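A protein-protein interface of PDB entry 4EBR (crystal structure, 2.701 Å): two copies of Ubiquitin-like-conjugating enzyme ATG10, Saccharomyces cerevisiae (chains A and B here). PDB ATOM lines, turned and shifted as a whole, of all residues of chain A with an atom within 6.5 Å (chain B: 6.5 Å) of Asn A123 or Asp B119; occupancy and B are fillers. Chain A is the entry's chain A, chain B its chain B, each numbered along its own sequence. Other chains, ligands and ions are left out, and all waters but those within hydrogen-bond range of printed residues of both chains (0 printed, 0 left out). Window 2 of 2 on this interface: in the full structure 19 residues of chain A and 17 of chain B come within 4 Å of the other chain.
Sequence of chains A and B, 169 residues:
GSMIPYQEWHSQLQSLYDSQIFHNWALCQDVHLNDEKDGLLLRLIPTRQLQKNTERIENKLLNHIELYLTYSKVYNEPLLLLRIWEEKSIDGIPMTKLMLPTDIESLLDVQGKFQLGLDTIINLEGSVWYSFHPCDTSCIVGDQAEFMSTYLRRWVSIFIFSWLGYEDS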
ATOM      1  N   THR A 120     -20.887  -3.266  21.778  1.00  0.00           N
ATOM      2  CA  THR A 120     -21.028  -4.637  21.345  1.00  0.00           C
ATOM      3  C   THR A 120     -20.121  -5.541  22.139  1.00  0.00           C
ATOM      4  O   THR A 120     -18.917  -5.340  22.210  1.00  0.00           O
ATOM      5  CB  THR A 120     -20.684  -4.775  19.867  1.00  0.00           C
ATOM      6  OG1 THR A 120     -21.687  -4.113  19.103  1.00  0.00           O
ATOM      7  CG2 THR A 120     -20.661  -6.215  19.453  1.00  0.00           C
ATOM      8  N   ILE A 121     -20.725  -6.551  22.733  1.00  0.00           N
ATOM      9  CA  ILE A 121     -20.008  -7.490  23.550  1.00  0.00           C
ATOM     10  C   ILE A 121     -20.057  -8.779  22.774  1.00  0.00           C
ATOM     11  O   ILE A 121     -21.083  -9.117  22.192  1.00  0.00           O
ATOM     12  CB  ILE A 121     -20.714  -7.645  24.902  1.00  0.00           C
ATOM     13  CG1 ILE A 121     -20.596  -6.346  25.712  1.00  0.00           C
ATOM     14  CG2 ILE A 121     -20.180  -8.805  25.672  1.00  0.00           C
ATOM     15  CD1 ILE A 121     -21.847  -5.428  25.590  1.00  0.00           C
ATOM     16  N   ILE A 122     -18.932  -9.480  22.717  1.00  0.00           N
ATOM     17  CA  ILE A 122     -18.868 -10.744  22.000  1.00  0.00           C
ATOM     18  C   ILE A 122     -18.498 -11.854  22.968  1.00  0.00           C
ATOM     19  O   ILE A 122     -17.526 -11.737  23.713  1.00  0.00           O
ATOM     20  CB  ILE A 122     -17.833 -10.697  20.862  1.00  0.00           C
ATOM     21  CG1 ILE A 122     -18.273  -9.707  19.780  1.00  0.00           C
ATOM     22  CG2 ILE A 122     -17.629 -12.083  20.270  1.00  0.00           C
ATOM     23  CD1 ILE A 122     -17.200  -9.401  18.759  1.00  0.00           C
ATOM     24  N   ASN A 123     -19.272 -12.932  22.960  1.00  0.00           N
ATOM     25  CA  ASN A 123     -18.993 -14.029  23.859  1.00  0.00           C
ATOM     26  C   ASN A 123     -18.304 -15.177  23.129  1.00  0.00           C
ATOM     27  O   ASN A 123     -18.849 -15.740  22.177  1.00  0.00           O
ATOM     28  CB  ASN A 123     -20.287 -14.503  24.504  1.00  0.00           C
ATOM     29  CG  ASN A 123     -20.052 -15.540  25.584  1.00  0.00           C
ATOM     30  OD1 ASN A 123     -19.863 -16.733  25.296  1.00  0.00           O
ATOM     31  ND2 ASN A 123     -20.071 -15.091  26.849  1.00  0.00           N
ATOM     32  N   LEU A 124     -17.086 -15.475  23.554  1.00  0.00           N
ATOM     33  CA  LEU A 124     -16.376 -16.610  23.014  1.00  0.00           C
ATOM     34  C   LEU A 124     -16.352 -17.662  24.100  1.00  0.00           C
ATOM     35  O   LEU A 124     -15.780 -17.460  25.171  1.00  0.00           O
ATOM     36  CB  LEU A 124     -14.952 -16.220  22.620  1.00  0.00           C
ATOM     37  CG  LEU A 124     -14.818 -15.200  21.487  1.00  0.00           C
ATOM     38  CD1 LEU A 124     -13.369 -14.770  21.320  1.00  0.00           C
ATOM     39  CD2 LEU A 124     -15.366 -15.766  20.186  1.00  0.00           C
ATOM     40  N   GLU A 125     -16.974 -18.793  23.809  1.00  0.00           N
ATOM     41  CA  GLU A 125     -16.949 -19.929  24.716  1.00  0.00           C
ATOM     42  C   GLU A 125     -16.952 -19.498  26.174  1.00  0.00           C
ATOM     43  O   GLU A 125     -16.192 -20.017  26.974  1.00  0.00           O
ATOM     44  CB  GLU A 125     -15.764 -20.847  24.391  1.00  0.00           C
ATOM     45  CG  GLU A 125     -15.931 -21.553  23.044  1.00  0.00           C
ATOM     46  CD  GLU A 125     -14.877 -22.614  22.771  1.00  0.00           C
ATOM     47  OE1 GLU A 125     -14.769 -23.584  23.569  1.00  0.00           O
ATOM     48  OE2 GLU A 125     -14.164 -22.479  21.746  1.00  0.00           O
ATOM     49  N   GLY A 126     -17.779 -18.513  26.506  1.00  0.00           N
ATOM     50  CA  GLY A 126     -17.891 -18.046  27.879  1.00  0.00           C
ATOM     51  C   GLY A 126     -17.039 -16.841  28.245  1.00  0.00           C
ATOM     52  O   GLY A 126     -17.287 -16.187  29.259  1.00  0.00           O
ATOM     53  N   SER A 127     -16.012 -16.554  27.454  1.00  0.00           N
ATOM     54  CA  SER A 127     -15.226 -15.362  27.702  1.00  0.00           C
ATOM     55  C   SER A 127     -15.892 -14.164  27.029  1.00  0.00           C
ATOM     56  O   SER A 127     -16.572 -14.323  26.016  1.00  0.00           O
ATOM     57  CB  SER A 127     -13.784 -15.556  27.266  1.00  0.00           C
ATOM     58  OG  SER A 127     -13.703 -15.789  25.882  1.00  0.00           O
ATOM     59  N   VAL A 128     -15.733 -12.982  27.617  1.00  0.00           N
ATOM     60  CA  VAL A 128     -16.419 -11.773  27.156  1.00  0.00           C
ATOM     61  C   VAL A 128     -15.481 -10.773  26.476  1.00  0.00           C
ATOM     62  O   VAL A 128     -14.511 -10.324  27.060  1.00  0.00           O
ATOM     63  CB  VAL A 128     -17.118 -11.061  28.333  1.00  0.00           C
ATOM     64  CG1 VAL A 128     -17.605  -9.669  27.932  1.00  0.00           C
ATOM     65  CG2 VAL A 128     -18.226 -11.882  28.818  1.00  0.00           C
ATOM     66  N   TRP A 129     -15.780 -10.414  25.240  1.00  0.00           N
ATOM     67  CA  TRP A 129     -14.908  -9.500  24.509  1.00  0.00           C
ATOM     68  C   TRP A 129     -15.675  -8.281  24.030  1.00  0.00           C
ATOM     69  O   TRP A 129     -16.868  -8.369  23.673  1.00  0.00           O
ATOM     70  CB  TRP A 129     -14.286 -10.200  23.313  1.00  0.00           C
ATOM     71  CG  TRP A 129     -13.442 -11.367  23.673  1.00  0.00           C
ATOM     72  CD1 TRP A 129     -13.870 -12.611  24.043  1.00  0.00           C
ATOM     73  CD2 TRP A 129     -12.011 -11.414  23.679  1.00  0.00           C
ATOM     74  NE1 TRP A 129     -12.791 -13.431  24.288  1.00  0.00           N
ATOM     75  CE2 TRP A 129     -11.638 -12.725  24.071  1.00  0.00           C
ATOM     76  CE3 TRP A 129     -11.010 -10.482  23.385  1.00  0.00           C
ATOM     77  CZ2 TRP A 129     -10.314 -13.122  24.175  1.00  0.00           C
ATOM     78  CZ3 TRP A 129      -9.694 -10.875  23.490  1.00  0.00           C
ATOM     79  CH2 TRP A 129      -9.356 -12.190  23.883  1.00  0.00           C
ATOM     80  N   PRO B 101     -29.923 -15.560  26.378  1.00  0.00           N
ATOM     81  CA  PRO B 101     -29.684 -15.867  24.960  1.00  0.00           C
ATOM     82  C   PRO B 101     -29.753 -17.352  24.617  1.00  0.00           C
ATOM     83  O   PRO B 101     -30.374 -17.705  23.613  1.00  0.00           O
ATOM     84  CB  PRO B 101     -28.261 -15.350  24.721  1.00  0.00           C
ATOM     85  CG  PRO B 101     -27.620 -15.401  26.042  1.00  0.00           C
ATOM     86  CD  PRO B 101     -28.714 -15.017  27.016  1.00  0.00           C
ATOM     87  N   THR B 102     -29.139 -18.204  25.426  1.00  0.00           N
ATOM     88  CA  THR B 102     -29.113 -19.632  25.118  1.00  0.00           C
ATOM     89  C   THR B 102     -30.528 -20.210  25.016  1.00  0.00           C
ATOM     90  O   THR B 102     -30.773 -21.157  24.256  1.00  0.00           O
ATOM     91  CB  THR B 102     -28.259 -20.438  26.130  1.00  0.00           C
ATOM     92  OG1 THR B 102     -28.589 -20.038  27.470  1.00  0.00           O
ATOM     93  CG2 THR B 102     -26.760 -20.207  25.866  1.00  0.00           C
ATOM     94  N   GLU B 105     -32.002 -19.052  21.851  1.00  0.00           N
ATOM     95  CA  GLU B 105     -31.470 -19.978  20.873  1.00  0.00           C
ATOM     96  C   GLU B 105     -32.261 -21.261  20.816  1.00  0.00           C
ATOM     97  O   GLU B 105     -32.275 -21.915  19.795  1.00  0.00           O
ATOM     98  CB  GLU B 105     -30.017 -20.301  21.174  1.00  0.00           C
ATOM     99  CG  GLU B 105     -29.048 -19.319  20.570  1.00  0.00           C
ATOM    100  CD  GLU B 105     -27.637 -19.503  21.098  1.00  0.00           C
ATOM    101  OE1 GLU B 105     -27.382 -20.504  21.814  1.00  0.00           O
ATOM    102  OE2 GLU B 105     -26.788 -18.633  20.802  1.00  0.00           O
ATOM    103  N   GLN B 115     -27.985 -20.105  13.826  1.00  0.00           N
ATOM    104  CA  GLN B 115     -27.679 -18.717  14.159  1.00  0.00           C
ATOM    105  C   GLN B 115     -26.223 -18.467  13.766  1.00  0.00           C
ATOM    106  O   GLN B 115     -25.319 -19.219  14.151  1.00  0.00           O
ATOM    107  CB  GLN B 115     -27.981 -18.354  15.620  1.00  0.00           C
ATOM    108  CG  GLN B 115     -27.090 -18.997  16.674  1.00  0.00           C
ATOM    109  CD  GLN B 115     -27.553 -20.387  17.041  1.00  0.00           C
ATOM    110  OE1 GLN B 115     -28.375 -20.982  16.344  1.00  0.00           O
ATOM    111  NE2 GLN B 115     -27.031 -20.913  18.142  1.00  0.00           N
ATOM    112  N   LEU B 116     -26.040 -17.480  12.897  1.00  0.00           N
ATOM    113  CA  LEU B 116     -24.752 -17.188  12.281  1.00  0.00           C
ATOM    114  C   LEU B 116     -23.739 -16.509  13.194  1.00  0.00           C
ATOM    115  O   LEU B 116     -24.098 -15.734  14.080  1.00  0.00           O
ATOM    116  CB  LEU B 116     -24.950 -16.346  11.015  1.00  0.00           C
ATOM    117  CG  LEU B 116     -25.696 -17.021   9.863  1.00  0.00           C
ATOM    118  CD1 LEU B 116     -25.947 -16.033   8.734  1.00  0.00           C
ATOM    119  CD2 LEU B 116     -24.928 -18.233   9.361  1.00  0.00           C
ATOM    120  N   GLY B 117     -22.466 -16.800  12.949  1.00  0.00           N
ATOM    121  CA  GLY B 117     -21.372 -16.042  13.532  1.00  0.00           C
ATOM    122  C   GLY B 117     -21.145 -16.197  15.025  1.00  0.00           C
ATOM    123  O   GLY B 117     -21.260 -17.295  15.574  1.00  0.00           O
ATOM    124  N   LEU B 118     -20.826 -15.084  15.679  1.00  0.00           N
ATOM    125  CA  LEU B 118     -20.457 -15.102  17.085  1.00  0.00           C
ATOM    126  C   LEU B 118     -21.572 -14.489  17.929  1.00  0.00           C
ATOM    127  O   LEU B 118     -22.349 -13.664  17.440  1.00  0.00           O
ATOM    128  CB  LEU B 118     -19.137 -14.366  17.309  1.00  0.00           C
ATOM    129  CG  LEU B 118     -17.904 -14.977  16.632  1.00  0.00           C
ATOM    130  CD1 LEU B 118     -16.624 -14.209  16.966  1.00  0.00           C
ATOM    131  CD2 LEU B 118     -17.762 -16.449  17.008  1.00  0.00           C
ATOM    132  N   ASP B 119     -21.676 -14.934  19.177  1.00  0.00           N
ATOM    133  CA  ASP B 119     -22.727 -14.440  20.045  1.00  0.00           C
ATOM    134  C   ASP B 119     -22.471 -12.959  20.195  1.00  0.00           C
ATOM    135  O   ASP B 119     -21.329 -12.536  20.372  1.00  0.00           O
ATOM    136  CB  ASP B 119     -22.673 -15.132  21.407  1.00  0.00           C
ATOM    137  CG  ASP B 119     -23.287 -16.517  21.381  1.00  0.00           C
ATOM    138  OD1 ASP B 119     -23.946 -16.859  20.377  1.00  0.00           O
ATOM    139  OD2 ASP B 119     -23.112 -17.265  22.366  1.00  0.00           O
ATOM    140  N   THR B 120     -23.527 -12.162  20.115  1.00  0.00           N
ATOM    141  CA  THR B 120     -23.341 -10.736  20.128  1.00  0.00           C
ATOM    142  C   THR B 120     -24.426 -10.027  20.899  1.00  0.00           C
ATOM    143  O   THR B 120     -25.578  -9.961  20.487  1.00  0.00           O
ATOM    144  CB  THR B 120     -23.318 -10.219  18.703  1.00  0.00           C
ATOM    145  OG1 THR B 120     -22.237 -10.841  18.021  1.00  0.00           O
ATOM    146  CG2 THR B 120     -23.100  -8.742  18.678  1.00  0.00           C
ATOM    147  N   ILE B 121     -24.037  -9.466  22.022  1.00  0.00           N
ATOM    148  CA  ILE B 121     -24.959  -8.734  22.850  1.00  0.00           C
ATOM    149  C   ILE B 121     -24.737  -7.283  22.489  1.00  0.00           C
ATOM    150  O   ILE B 121     -23.591  -6.835  22.380  1.00  0.00           O
ATOM    151  CB  ILE B 121     -24.650  -8.949  24.336  1.00  0.00           C
ATOM    152  CG1 ILE B 121     -24.717 -10.428  24.682  1.00  0.00           C
ATOM    153  CG2 ILE B 121     -25.613  -8.202  25.193  1.00  0.00           C
ATOM    154  CD1 ILE B 121     -23.317 -11.099  24.754  1.00  0.00           C
ATOM    155  N   TYR B 130     -30.022  -8.877  21.754  1.00  0.00           N
ATOM    156  CA  TYR B 130     -29.424  -9.953  20.979  1.00  0.00           C
ATOM    157  C   TYR B 130     -29.309  -9.501  19.537  1.00  0.00           C
ATOM    158  O   TYR B 130     -30.288  -9.036  18.946  1.00  0.00           O
ATOM    159  CB  TYR B 130     -30.369 -11.147  21.026  1.00  0.00           C
ATOM    160  CG  TYR B 130     -29.833 -12.448  20.489  1.00  0.00           C
ATOM    161  CD1 TYR B 130     -28.782 -13.091  21.100  1.00  0.00           C
ATOM    162  CD2 TYR B 130     -30.414 -13.062  19.396  1.00  0.00           C
ATOM    163  CE1 TYR B 130     -28.316 -14.296  20.626  1.00  0.00           C
ATOM    164  CE2 TYR B 130     -29.945 -14.266  18.919  1.00  0.00           C
ATOM    165  CZ  TYR B 130     -28.902 -14.869  19.545  1.00  0.00           C
ATOM    166  OH  TYR B 130     -28.414 -16.050  19.093  1.00  0.00           O
ATOM    167  N   SER B 131     -28.124  -9.625  18.955  1.00  0.00           N
ATOM    168  CA  SER B 131     -28.017  -9.380  17.532  1.00  0.00           C
ATOM    169  C   SER B 131     -28.586 -10.596  16.787  1.00  0.00           C
ATOM    170  O   SER B 131     -28.091 -11.707  16.929  1.00  0.00           O
ATOM    171  CB  SER B 131     -26.539  -9.215  17.204  1.00  0.00           C
ATOM    172  OG  SER B 131     -26.381  -8.730  15.892  1.00  0.00           O
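The backbone carbonyl oxygen (O) of Ile B121 is in hydrogen-bond range of the backbone NH (N) of Ile A121, 2.9 Å away. The backbone NH (N) of Asn A123 sits at hydrogen-bond distance from the backbone carbonyl oxygen (O) of Asp B119 (3.3 Å).
N of Ile A122 sits at hydrogen-bond distance from O of Trp A129, at 2.5 Å. The backbone NH (N) of Gly A126 is in hydrogen-bond range of the side-chain amide oxygen (OD1) of Asn A123, 3.0 Å away. OG of Ser A127 sits at hydrogen-bond distance from O of Leu A124 (2.8 Å). The backbone carbonyl oxygen of Leu B118 is in hydrogen-bond range of the side-chain hydroxyl of Thr B120 (2.9 Å). The backbone NH (N) of Ser B131 sits at hydrogen-bond distance from the backbone carbonyl oxygen (O) of Thr B120 (3.0 Å).
Among the printed residues, pairs that only touch across the chains: Ile A122 with Asp B119 (3.5 Å), Ile A121 with Thr B120 (3.5 Å), Thr A120 with Ile B121 (3.5 Å), Thr A120 with Thr B120 (3.6 Å), Leu A124 with Leu B118 (3.8 Å) and Ile A121 with Asp B119 (3.9 Å).
Of the printed residues of chain B, Thr A120 touches Thr B120 (3.6 Å) and Ile B121 (3.5 Å). Of the printed residues of chain B, Ile A121 touches Asp B119, Thr B120 and Ile B121. Of the printed residues of chain B, Ile A122 touches Asp B119. Printed residues of chain B within 4 Å of Leu A124: Leu B118 (3.8 Å). Gly A126 touches none of the printed residues of chain B. Ser A127 touches none of the printed residues of chain B. Of chain A, only Ile A121, Ile A122 and Asn A123 come within 4 Å of Asp B119. Of the printed residues of chain A, Ile B121 touches Thr A120 and Ile A121. The nearest residue of chain B that does not touch Asn A123 is Ile B121 (4.6 Å). The nearest printed residue of chain B that does not touch Ile A121 is Leu B118 (6.7 Å).
Of the 12 printed residues of chain B, 4 touch a printed residue of chain A. Hydrophobic or aromatic side chains of chain B within 4 Å of the printed part of chain A: Leu B118 and Ile B121. Along chain B the printed residues that touch a printed residue of chain A span positions 118 to 121. Hydrophobic or aromatic side chains of chain A that line the printed part of chain B: Ile A121, Ile A122 and Leu A124. Among the printed residues, no Asp or Glu carboxylate lies within 4 Å of a Lys or Arg side-chain nitrogen of the other chain.
Thr A120 touches its own counterpart, Thr B120. Thr A120 touches Ile B121, and with the chains exchanged Ile A121 touches Thr B120. Ile A121 touches its own counterpart, Ile B121. Positions printed for both chains: 120 and 121.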
